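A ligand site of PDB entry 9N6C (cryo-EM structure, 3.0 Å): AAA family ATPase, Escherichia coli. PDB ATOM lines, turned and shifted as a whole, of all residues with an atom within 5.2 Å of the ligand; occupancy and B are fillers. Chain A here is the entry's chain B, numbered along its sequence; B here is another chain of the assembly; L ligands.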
ATOM      1  N   LYS A  64     -18.452  32.111   6.327  1.00  0.00           N
ATOM      2  CA  LYS A  64     -18.942  30.819   5.863  1.00  0.00           C
ATOM      3  C   LYS A  64     -19.197  29.852   7.019  1.00  0.00           C
ATOM      4  O   LYS A  64     -20.112  30.076   7.829  1.00  0.00           O
ATOM      5  CB  LYS A  64     -17.972  30.203   4.864  1.00  0.00           C
ATOM      6  CG  LYS A  64     -18.018  30.854   3.491  1.00  0.00           C
ATOM      7  CD  LYS A  64     -17.578  29.898   2.398  1.00  0.00           C
ATOM      8  CE  LYS A  64     -16.900  30.649   1.264  1.00  0.00           C
ATOM      9  NZ  LYS A  64     -16.094  29.734   0.399  1.00  0.00           N
ATOM     10  N   ARG A  65     -18.410  28.790   7.102  1.00  0.00           N
ATOM     11  CA  ARG A  65     -18.677  27.711   8.043  1.00  0.00           C
ATOM     12  C   ARG A  65     -18.066  27.952   9.416  1.00  0.00           C
ATOM     13  O   ARG A  65     -18.398  27.232  10.367  1.00  0.00           O
ATOM     14  CB  ARG A  65     -18.149  26.381   7.486  1.00  0.00           C
ATOM     15  CG  ARG A  65     -18.655  25.138   8.218  1.00  0.00           C
ATOM     16  CD  ARG A  65     -17.511  24.219   8.578  1.00  0.00           C
ATOM     17  NE  ARG A  65     -17.916  23.223   9.568  1.00  0.00           N
ATOM     18  CZ  ARG A  65     -18.447  22.041   9.279  1.00  0.00           C
ATOM     19  NH1 ARG A  65     -18.670  21.680   8.033  1.00  0.00           N
ATOM     20  NH2 ARG A  65     -18.762  21.210  10.270  1.00  0.00           N
ATOM     21  N   ASP A  83     -11.073  16.560   5.942  1.00  0.00           N
ATOM     22  CA  ASP A  83     -11.983  15.971   4.982  1.00  0.00           C
ATOM     23  C   ASP A  83     -12.809  17.062   4.305  1.00  0.00           C
ATOM     24  O   ASP A  83     -12.719  18.247   4.639  1.00  0.00           O
ATOM     25  CB  ASP A  83     -12.883  14.939   5.660  1.00  0.00           C
ATOM     26  CG  ASP A  83     -12.097  13.888   6.409  1.00  0.00           C
ATOM     27  OD1 ASP A  83     -11.558  14.206   7.490  1.00  0.00           O
ATOM     28  OD2 ASP A  83     -12.021  12.738   5.918  1.00  0.00           O
ATOM     29  N   ASN A  84     -13.620  16.645   3.332  1.00  0.00           N
ATOM     30  CA  ASN A  84     -14.508  17.584   2.648  1.00  0.00           C
ATOM     31  C   ASN A  84     -15.482  18.215   3.632  1.00  0.00           C
ATOM     32  O   ASN A  84     -16.090  17.525   4.454  1.00  0.00           O
ATOM     33  CB  ASN A  84     -15.271  16.858   1.542  1.00  0.00           C
ATOM     34  CG  ASN A  84     -14.386  16.432   0.391  1.00  0.00           C
ATOM     35  OD1 ASN A  84     -14.287  17.115  -0.625  1.00  0.00           O
ATOM     36  ND2 ASN A  84     -13.726  15.292   0.548  1.00  0.00           N
ATOM     37  N   GLY A  85     -15.634  19.534   3.543  1.00  0.00           N
ATOM     38  CA  GLY A  85     -16.521  20.235   4.445  1.00  0.00           C
ATOM     39  C   GLY A  85     -15.875  20.571   5.771  1.00  0.00           C
ATOM     40  O   GLY A  85     -16.458  20.312   6.830  1.00  0.00           O
ATOM     41  N   PHE A  86     -14.668  21.163   5.742  1.00  0.00           N
ATOM     42  CA  PHE A  86     -14.000  21.517   6.987  1.00  0.00           C
ATOM     43  C   PHE A  86     -13.346  22.887   6.938  1.00  0.00           C
ATOM     44  O   PHE A  86     -12.510  23.194   7.801  1.00  0.00           O
ATOM     45  CB  PHE A  86     -12.951  20.461   7.335  1.00  0.00           C
ATOM     46  CG  PHE A  86     -13.472  19.352   8.210  1.00  0.00           C
ATOM     47  CD1 PHE A  86     -14.367  19.624   9.236  1.00  0.00           C
ATOM     48  CD2 PHE A  86     -13.071  18.045   8.011  1.00  0.00           C
ATOM     49  CE1 PHE A  86     -14.846  18.612  10.032  1.00  0.00           C
ATOM     50  CE2 PHE A  86     -13.560  17.031   8.808  1.00  0.00           C
ATOM     51  CZ  PHE A  86     -14.446  17.311   9.820  1.00  0.00           C
ATOM     52  N   GLY A  87     -13.689  23.734   5.972  1.00  0.00           N
ATOM     53  CA  GLY A  87     -13.101  25.057   5.911  1.00  0.00           C
ATOM     54  C   GLY A  87     -11.684  25.122   5.396  1.00  0.00           C
ATOM     55  O   GLY A  87     -10.992  26.116   5.631  1.00  0.00           O
ATOM     56  N   LYS A  88     -11.223  24.083   4.693  1.00  0.00           N
ATOM     57  CA  LYS A  88      -9.854  24.060   4.190  1.00  0.00           C
ATOM     58  C   LYS A  88      -9.606  25.159   3.167  1.00  0.00           C
ATOM     59  O   LYS A  88      -8.543  25.798   3.179  1.00  0.00           O
ATOM     60  CB  LYS A  88      -9.555  22.684   3.604  1.00  0.00           C
ATOM     61  CG  LYS A  88      -8.158  22.167   3.842  1.00  0.00           C
ATOM     62  CD  LYS A  88      -8.135  20.644   3.892  1.00  0.00           C
ATOM     63  CE  LYS A  88      -8.891  19.998   2.735  1.00  0.00           C
ATOM     64  NZ  LYS A  88      -8.575  20.616   1.416  1.00  0.00           N
ATOM     65  N   SER A  89     -10.554  25.389   2.263  1.00  0.00           N
ATOM     66  CA  SER A  89     -10.376  26.393   1.214  1.00  0.00           C
ATOM     67  C   SER A  89     -10.843  27.786   1.618  1.00  0.00           C
ATOM     68  O   SER A  89     -10.481  28.763   0.955  1.00  0.00           O
ATOM     69  CB  SER A  89     -11.107  25.958  -0.053  1.00  0.00           C
ATOM     70  OG  SER A  89     -10.235  25.246  -0.919  1.00  0.00           O
ATOM     71  N   THR A  90     -11.562  27.913   2.733  1.00  0.00           N
ATOM     72  CA  THR A  90     -11.958  29.242   3.170  1.00  0.00           C
ATOM     73  C   THR A  90     -10.792  29.991   3.777  1.00  0.00           C
ATOM     74  O   THR A  90     -10.714  31.219   3.638  1.00  0.00           O
ATOM     75  CB  THR A  90     -13.089  29.146   4.198  1.00  0.00           C
ATOM     76  OG1 THR A  90     -12.768  28.150   5.176  1.00  0.00           O
ATOM     77  CG2 THR A  90     -14.377  28.756   3.507  1.00  0.00           C
ATOM     78  N   HIS A 119     -23.556  36.188  -0.411  1.00  0.00           N
ATOM     79  CA  HIS A 119     -23.811  34.774  -0.115  1.00  0.00           C
ATOM     80  C   HIS A 119     -22.726  34.156   0.755  1.00  0.00           C
ATOM     81  O   HIS A 119     -22.963  33.114   1.363  1.00  0.00           O
ATOM     82  CB  HIS A 119     -23.953  33.980  -1.409  1.00  0.00           C
ATOM     83  CG  HIS A 119     -22.656  33.635  -2.059  1.00  0.00           C
ATOM     84  ND1 HIS A 119     -22.021  34.477  -2.948  1.00  0.00           N
ATOM     85  CD2 HIS A 119     -21.863  32.539  -1.954  1.00  0.00           C
ATOM     86  CE1 HIS A 119     -20.891  33.911  -3.364  1.00  0.00           C
ATOM     87  NE2 HIS A 119     -20.778  32.734  -2.772  1.00  0.00           N
ATOM     88  N   GLU A 120     -21.544  34.773   0.835  1.00  0.00           N
ATOM     89  CA  GLU A 120     -20.461  34.201   1.624  1.00  0.00           C
ATOM     90  C   GLU A 120     -20.645  34.407   3.120  1.00  0.00           C
ATOM     91  O   GLU A 120     -20.002  33.712   3.904  1.00  0.00           O
ATOM     92  CB  GLU A 120     -19.114  34.801   1.194  1.00  0.00           C
ATOM     93  CG  GLU A 120     -18.511  34.153  -0.038  1.00  0.00           C
ATOM     94  CD  GLU A 120     -17.493  35.041  -0.721  1.00  0.00           C
ATOM     95  OE1 GLU A 120     -17.789  36.231  -0.929  1.00  0.00           O
ATOM     96  OE2 GLU A 120     -16.393  34.541  -1.032  1.00  0.00           O
ATOM     97  N   VAL A 121     -21.509  35.341   3.522  1.00  0.00           N
ATOM     98  CA  VAL A 121     -21.730  35.559   4.950  1.00  0.00           C
ATOM     99  C   VAL A 121     -22.475  34.366   5.533  1.00  0.00           C
ATOM    100  O   VAL A 121     -23.185  33.632   4.832  1.00  0.00           O
ATOM    101  CB  VAL A 121     -22.514  36.870   5.171  1.00  0.00           C
ATOM    102  CG1 VAL A 121     -22.306  37.375   6.588  1.00  0.00           C
ATOM    103  CG2 VAL A 121     -22.086  37.916   4.162  1.00  0.00           C
ATOM    104  N   ASN A 122     -22.308  34.163   6.846  1.00  0.00           N
ATOM    105  CA  ASN A 122     -22.966  33.059   7.522  1.00  0.00           C
ATOM    106  C   ASN A 122     -24.478  33.220   7.448  1.00  0.00           C
ATOM    107  O   ASN A 122     -25.007  34.330   7.509  1.00  0.00           O
ATOM    108  CB  ASN A 122     -22.511  32.981   8.972  1.00  0.00           C
ATOM    109  CG  ASN A 122     -22.636  31.592   9.552  1.00  0.00           C
ATOM    110  OD1 ASN A 122     -23.734  31.017   9.583  1.00  0.00           O
ATOM    111  ND2 ASN A 122     -21.530  31.033  10.007  1.00  0.00           N
ATOM    112  N   ASN A 123     -25.176  32.090   7.315  1.00  0.00           N
ATOM    113  CA  ASN A 123     -26.631  32.084   7.171  1.00  0.00           C
ATOM    114  C   ASN A 123     -27.358  32.010   8.508  1.00  0.00           C
ATOM    115  O   ASN A 123     -28.583  31.871   8.523  1.00  0.00           O
ATOM    116  CB  ASN A 123     -27.067  30.909   6.291  1.00  0.00           C
ATOM    117  CG  ASN A 123     -26.289  30.834   4.995  1.00  0.00           C
ATOM    118  OD1 ASN A 123     -25.754  31.840   4.519  1.00  0.00           O
ATOM    119  ND2 ASN A 123     -26.214  29.640   4.414  1.00  0.00           N
ATOM    120  N   ASP A 395      -3.582  24.549  -3.197  1.00  0.00           N
ATOM    121  CA  ASP A 395      -4.748  23.824  -2.717  1.00  0.00           C
ATOM    122  C   ASP A 395      -4.802  22.465  -3.405  1.00  0.00           C
ATOM    123  O   ASP A 395      -4.746  22.389  -4.634  1.00  0.00           O
ATOM    124  CB  ASP A 395      -6.030  24.616  -2.984  1.00  0.00           C
ATOM    125  CG  ASP A 395      -7.237  24.016  -2.314  1.00  0.00           C
ATOM    126  OD1 ASP A 395      -7.070  23.122  -1.464  1.00  0.00           O
ATOM    127  OD2 ASP A 395      -8.366  24.431  -2.651  1.00  0.00           O
ATOM    128  N   GLU A 396      -4.920  21.403  -2.602  1.00  0.00           N
ATOM    129  CA  GLU A 396      -5.059  20.025  -3.099  1.00  0.00           C
ATOM    130  C   GLU A 396      -3.878  19.648  -4.000  1.00  0.00           C
ATOM    131  O   GLU A 396      -4.012  19.414  -5.198  1.00  0.00           O
ATOM    132  CB  GLU A 396      -6.397  19.851  -3.823  1.00  0.00           C
ATOM    133  CG  GLU A 396      -7.572  19.636  -2.900  1.00  0.00           C
ATOM    134  CD  GLU A 396      -8.599  18.682  -3.479  1.00  0.00           C
ATOM    135  OE1 GLU A 396      -9.426  19.133  -4.297  1.00  0.00           O
ATOM    136  OE2 GLU A 396      -8.583  17.499  -3.105  1.00  0.00           O
ATOM    137  N   LYS B 347     -28.094  20.779   5.999  1.00  0.00           N
ATOM    138  CA  LYS B 347     -26.903  20.228   6.650  1.00  0.00           C
ATOM    139  C   LYS B 347     -26.964  20.576   8.132  1.00  0.00           C
ATOM    140  O   LYS B 347     -26.859  21.747   8.514  1.00  0.00           O
ATOM    141  CB  LYS B 347     -25.638  20.797   6.021  1.00  0.00           C
ATOM    142  CG  LYS B 347     -24.375  20.571   6.828  1.00  0.00           C
ATOM    143  CD  LYS B 347     -24.064  19.099   7.021  1.00  0.00           C
ATOM    144  CE  LYS B 347     -23.522  18.501   5.742  1.00  0.00           C
ATOM    145  NZ  LYS B 347     -22.303  19.224   5.292  1.00  0.00           N
ATOM    146  N   VAL B 350     -28.609  23.897   9.366  1.00  0.00           N
ATOM    147  CA  VAL B 350     -28.435  24.992   8.422  1.00  0.00           C
ATOM    148  C   VAL B 350     -29.020  24.565   7.084  1.00  0.00           C
ATOM    149  O   VAL B 350     -29.149  23.382   6.772  1.00  0.00           O
ATOM    150  CB  VAL B 350     -26.951  25.384   8.254  1.00  0.00           C
ATOM    151  CG1 VAL B 350     -26.833  26.836   7.821  1.00  0.00           C
ATOM    152  CG2 VAL B 350     -26.175  25.146   9.539  1.00  0.00           C
ATOM    153  N   LEU B 352     -28.623  25.264   2.893  1.00  0.00           N
ATOM    154  CA  LEU B 352     -27.701  25.751   1.879  1.00  0.00           C
ATOM    155  C   LEU B 352     -28.171  25.347   0.497  1.00  0.00           C
ATOM    156  O   LEU B 352     -28.714  24.245   0.317  1.00  0.00           O
ATOM    157  CB  LEU B 352     -26.275  25.232   2.096  1.00  0.00           C
ATOM    158  CG  LEU B 352     -25.674  25.257   3.504  1.00  0.00           C
ATOM    159  CD1 LEU B 352     -25.940  23.952   4.229  1.00  0.00           C
ATOM    160  CD2 LEU B 352     -24.188  25.534   3.431  1.00  0.00           C
ATOM    161  N   GLN B 356     -23.647  26.773  -2.737  1.00  0.00           N
ATOM    162  CA  GLN B 356     -22.914  26.930  -1.498  1.00  0.00           C
ATOM    163  C   GLN B 356     -22.260  25.632  -1.028  1.00  0.00           C
ATOM    164  O   GLN B 356     -21.686  25.591   0.054  1.00  0.00           O
ATOM    165  CB  GLN B 356     -23.849  27.472  -0.419  1.00  0.00           C
ATOM    166  CG  GLN B 356     -23.155  28.197   0.711  1.00  0.00           C
ATOM    167  CD  GLN B 356     -23.937  29.407   1.192  1.00  0.00           C
ATOM    168  OE1 GLN B 356     -23.365  30.344   1.739  1.00  0.00           O
ATOM    169  NE2 GLN B 356     -25.243  29.381   0.988  1.00  0.00           N
ATOM    170  N   LEU B 357     -22.350  24.569  -1.832  1.00  0.00           N
ATOM    171  CA  LEU B 357     -21.871  23.257  -1.415  1.00  0.00           C
ATOM    172  C   LEU B 357     -20.355  23.159  -1.587  1.00  0.00           C
ATOM    173  O   LEU B 357     -19.690  24.089  -2.062  1.00  0.00           O
ATOM    174  CB  LEU B 357     -22.582  22.165  -2.189  1.00  0.00           C
ATOM    175  CG  LEU B 357     -23.034  20.939  -1.401  1.00  0.00           C
ATOM    176  CD1 LEU B 357     -23.599  21.355  -0.055  1.00  0.00           C
ATOM    177  CD2 LEU B 357     -24.059  20.153  -2.201  1.00  0.00           C
ATOM    178  N   SER B 358     -19.798  22.023  -1.194  1.00  0.00           N
ATOM    179  CA  SER B 358     -18.369  21.762  -1.304  1.00  0.00           C
ATOM    180  C   SER B 358     -18.021  21.140  -2.654  1.00  0.00           C
ATOM    181  O   SER B 358     -18.878  20.607  -3.360  1.00  0.00           O
ATOM    182  CB  SER B 358     -17.894  20.845  -0.169  1.00  0.00           C
ATOM    183  OG  SER B 358     -16.537  20.475  -0.344  1.00  0.00           O
ATOM    184  N   GLN B 359     -16.735  21.224  -3.002  1.00  0.00           N
ATOM    185  CA  GLN B 359     -16.272  20.697  -4.284  1.00  0.00           C
ATOM    186  C   GLN B 359     -16.443  19.179  -4.378  1.00  0.00           C
ATOM    187  O   GLN B 359     -16.852  18.658  -5.421  1.00  0.00           O
ATOM    188  CB  GLN B 359     -14.801  21.077  -4.511  1.00  0.00           C
ATOM    189  CG  GLN B 359     -14.238  20.551  -5.806  1.00  0.00           C
ATOM    190  CD  GLN B 359     -14.714  21.348  -7.005  1.00  0.00           C
ATOM    191  OE1 GLN B 359     -15.130  22.494  -6.864  1.00  0.00           O
ATOM    192  NE2 GLN B 359     -14.637  20.737  -8.180  1.00  0.00           N
ATOM    193  N   GLY B 360     -16.119  18.462  -3.310  1.00  0.00           N
ATOM    194  CA  GLY B 360     -16.251  17.010  -3.323  1.00  0.00           C
ATOM    195  C   GLY B 360     -17.690  16.544  -3.471  1.00  0.00           C
ATOM    196  O   GLY B 360     -17.957  15.573  -4.185  1.00  0.00           O
ATOM    197  N   GLU B 361     -18.623  17.219  -2.802  1.00  0.00           N
ATOM    198  CA  GLU B 361     -20.020  16.809  -2.843  1.00  0.00           C
ATOM    199  C   GLU B 361     -20.656  17.095  -4.203  1.00  0.00           C
ATOM    200  O   GLU B 361     -21.566  16.357  -4.620  1.00  0.00           O
ATOM    201  CB  GLU B 361     -20.793  17.525  -1.737  1.00  0.00           C
ATOM    202  CG  GLU B 361     -20.421  17.027  -0.346  1.00  0.00           C
ATOM    203  CD  GLU B 361     -20.536  18.116   0.711  1.00  0.00           C
ATOM    204  OE1 GLU B 361     -20.753  19.290   0.336  1.00  0.00           O
ATOM    205  OE2 GLU B 361     -20.405  17.801   1.906  1.00  0.00           O
HETATM  206  P1  LIG L   1     -12.066  22.205  -0.899  1.00  0.00           P
HETATM  207  O1  LIG L   1     -12.376  20.865  -1.457  1.00  0.00           O
HETATM  208  O2  LIG L   1     -12.245  23.347  -1.891  1.00  0.00           O
HETATM  209  O3  LIG L   1     -10.665  22.299  -0.275  1.00  0.00           O
HETATM  210  P2  LIG L   1     -13.534  21.966   1.703  1.00  0.00           P
HETATM  211  O4  LIG L   1     -13.920  20.547   1.590  1.00  0.00           O
HETATM  212  O5  LIG L   1     -12.463  22.280   2.725  1.00  0.00           O
HETATM  213  O6  LIG L   1     -13.059  22.558   0.303  1.00  0.00           O
HETATM  214  P3  LIG L   1     -15.081  24.451   2.055  1.00  0.00           P
HETATM  215  O7  LIG L   1     -15.234  24.993   0.693  1.00  0.00           O
HETATM  216  O8  LIG L   1     -13.967  25.098   2.881  1.00  0.00           O
HETATM  217  O9  LIG L   1     -14.778  22.901   2.031  1.00  0.00           O
HETATM  218  O10 LIG L   1     -16.423  24.529   2.878  1.00  0.00           O
HETATM  219  C1  LIG L   1     -17.480  23.568   2.684  1.00  0.00           C
HETATM  220  C2  LIG L   1     -18.501  23.755   3.766  1.00  0.00           C
HETATM  221  O11 LIG L   1     -18.821  25.158   3.865  1.00  0.00           O
HETATM  222  C3  LIG L   1     -19.837  23.059   3.529  1.00  0.00           C
HETATM  223  O12 LIG L   1     -19.880  21.807   4.217  1.00  0.00           O
HETATM  224  C4  LIG L   1     -20.878  24.043   4.089  1.00  0.00           C
HETATM  225  O13 LIG L   1     -21.593  23.488   5.185  1.00  0.00           O
HETATM  226  C5  LIG L   1     -20.053  25.244   4.543  1.00  0.00           C
HETATM  227  N1  LIG L   1     -20.643  26.537   4.243  1.00  0.00           N
HETATM  228  C6  LIG L   1     -20.451  27.287   3.104  1.00  0.00           C
HETATM  229  N2  LIG L   1     -21.098  28.419   3.098  1.00  0.00           N
HETATM  230  C7  LIG L   1     -21.764  28.430   4.317  1.00  0.00           C
HETATM  231  C8  LIG L   1     -22.623  29.363   4.922  1.00  0.00           C
HETATM  232  N3  LIG L   1     -22.983  30.521   4.355  1.00  0.00           N
HETATM  233  N4  LIG L   1     -23.108  29.069   6.140  1.00  0.00           N
HETATM  234  C9  LIG L   1     -22.758  27.922   6.714  1.00  0.00           C
HETATM  235  N5  LIG L   1     -21.957  26.966   6.247  1.00  0.00           N
HETATM  236  C10 LIG L   1     -21.484  27.281   5.033  1.00  0.00           C
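OD1 of Asn 123 lies within hydrogen-bond range of N3 of the ligand.
The backbone NH (N) of Gly 85 sits at hydrogen-bond distance from an oxygen (O4) of the ligand, 2.8 Å away.
N of Gly 87 sits close to O8 of the ligand, at 3.4 Å.
The backbone NH of Lys 88 sits at hydrogen-bond distance from an oxygen (O5) of the ligand (2.9 Å).
The side-chain amide oxygen of Gln 356 of chain B is in hydrogen-bond range of a nitrogen (N3) of the ligand (2.6 Å).
An oxygen (O2) of the ligand sits at hydrogen-bond distance from the side-chain hydroxyl (OG) of Ser 89 (2.9 Å).
An oxygen (O4) of the ligand lies within hydrogen-bond range of the side-chain hydroxyl (OG) of Ser 358 of chain B, 3.3 Å away.
The side-chain amino group of Lys 88 lies within salt-bridge range of an oxygen (O3) of the ligand, at 3.2 Å.
N of Ser 89 sits at hydrogen-bond distance from O8 of the ligand (3.5 Å).
A nitrogen (N3) of the ligand sits at hydrogen-bond distance from the backbone carbonyl oxygen (O) of Val 121 (3.2 Å).
The side-chain amide oxygen (OD1) of Asn 123 sits close to the backbone carbonyl oxygen (O) of Val 121.
The side-chain hydroxyl of Thr 90 sits at hydrogen-bond distance from the backbone carbonyl oxygen of Gly 87, 2.7 Å away.
O of Lys 64 is in hydrogen-bond range of ND2 of Asn 122 (2.8 Å).
OE1 of Gln 356 of chain B sits close to O of His 119.
The backbone carbonyl oxygen (O) of Gly 85 is in hydrogen-bond range of the guanidinium group (NH1) of Arg 65, at 2.9 Å.
The side-chain hydroxyl (OG) of Ser 89 is in hydrogen-bond range of the side-chain carboxylate (OD2) of Asp 395 (2.7 Å).
The backbone NH (N) of Lys 64 sits at hydrogen-bond distance from the backbone carbonyl oxygen (O) of Glu 120 (3.3 Å).
The backbone NH (N) of Ser 358 of chain B sits at hydrogen-bond distance from the side-chain carboxylate (OE1) of Glu 361 of chain B, at 3.3 Å.
Residues that only touch the ligand: Asn 84 (3.2 Å), Lys 64 (3.6 Å), Leu 352 of chain B (3.6 Å), Arg 65 (3.7 Å), Lys 347 of chain B (3.7 Å), Thr 90 (3.7 Å), Asp 395 (3.9 Å), Phe 86 (3.9 Å), Gln 359 of chain B (3.9 Å) and His 119 (3.96 Å).
Hydrophobic or aromatic side chains within 4 Å of the ligand: Leu 352 of chain B.
Of the 26 residues printed, 18 come within 4 Å of the ligand.
Along chain A the residues within 4 Å of the ligand span positions 64 to 395.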
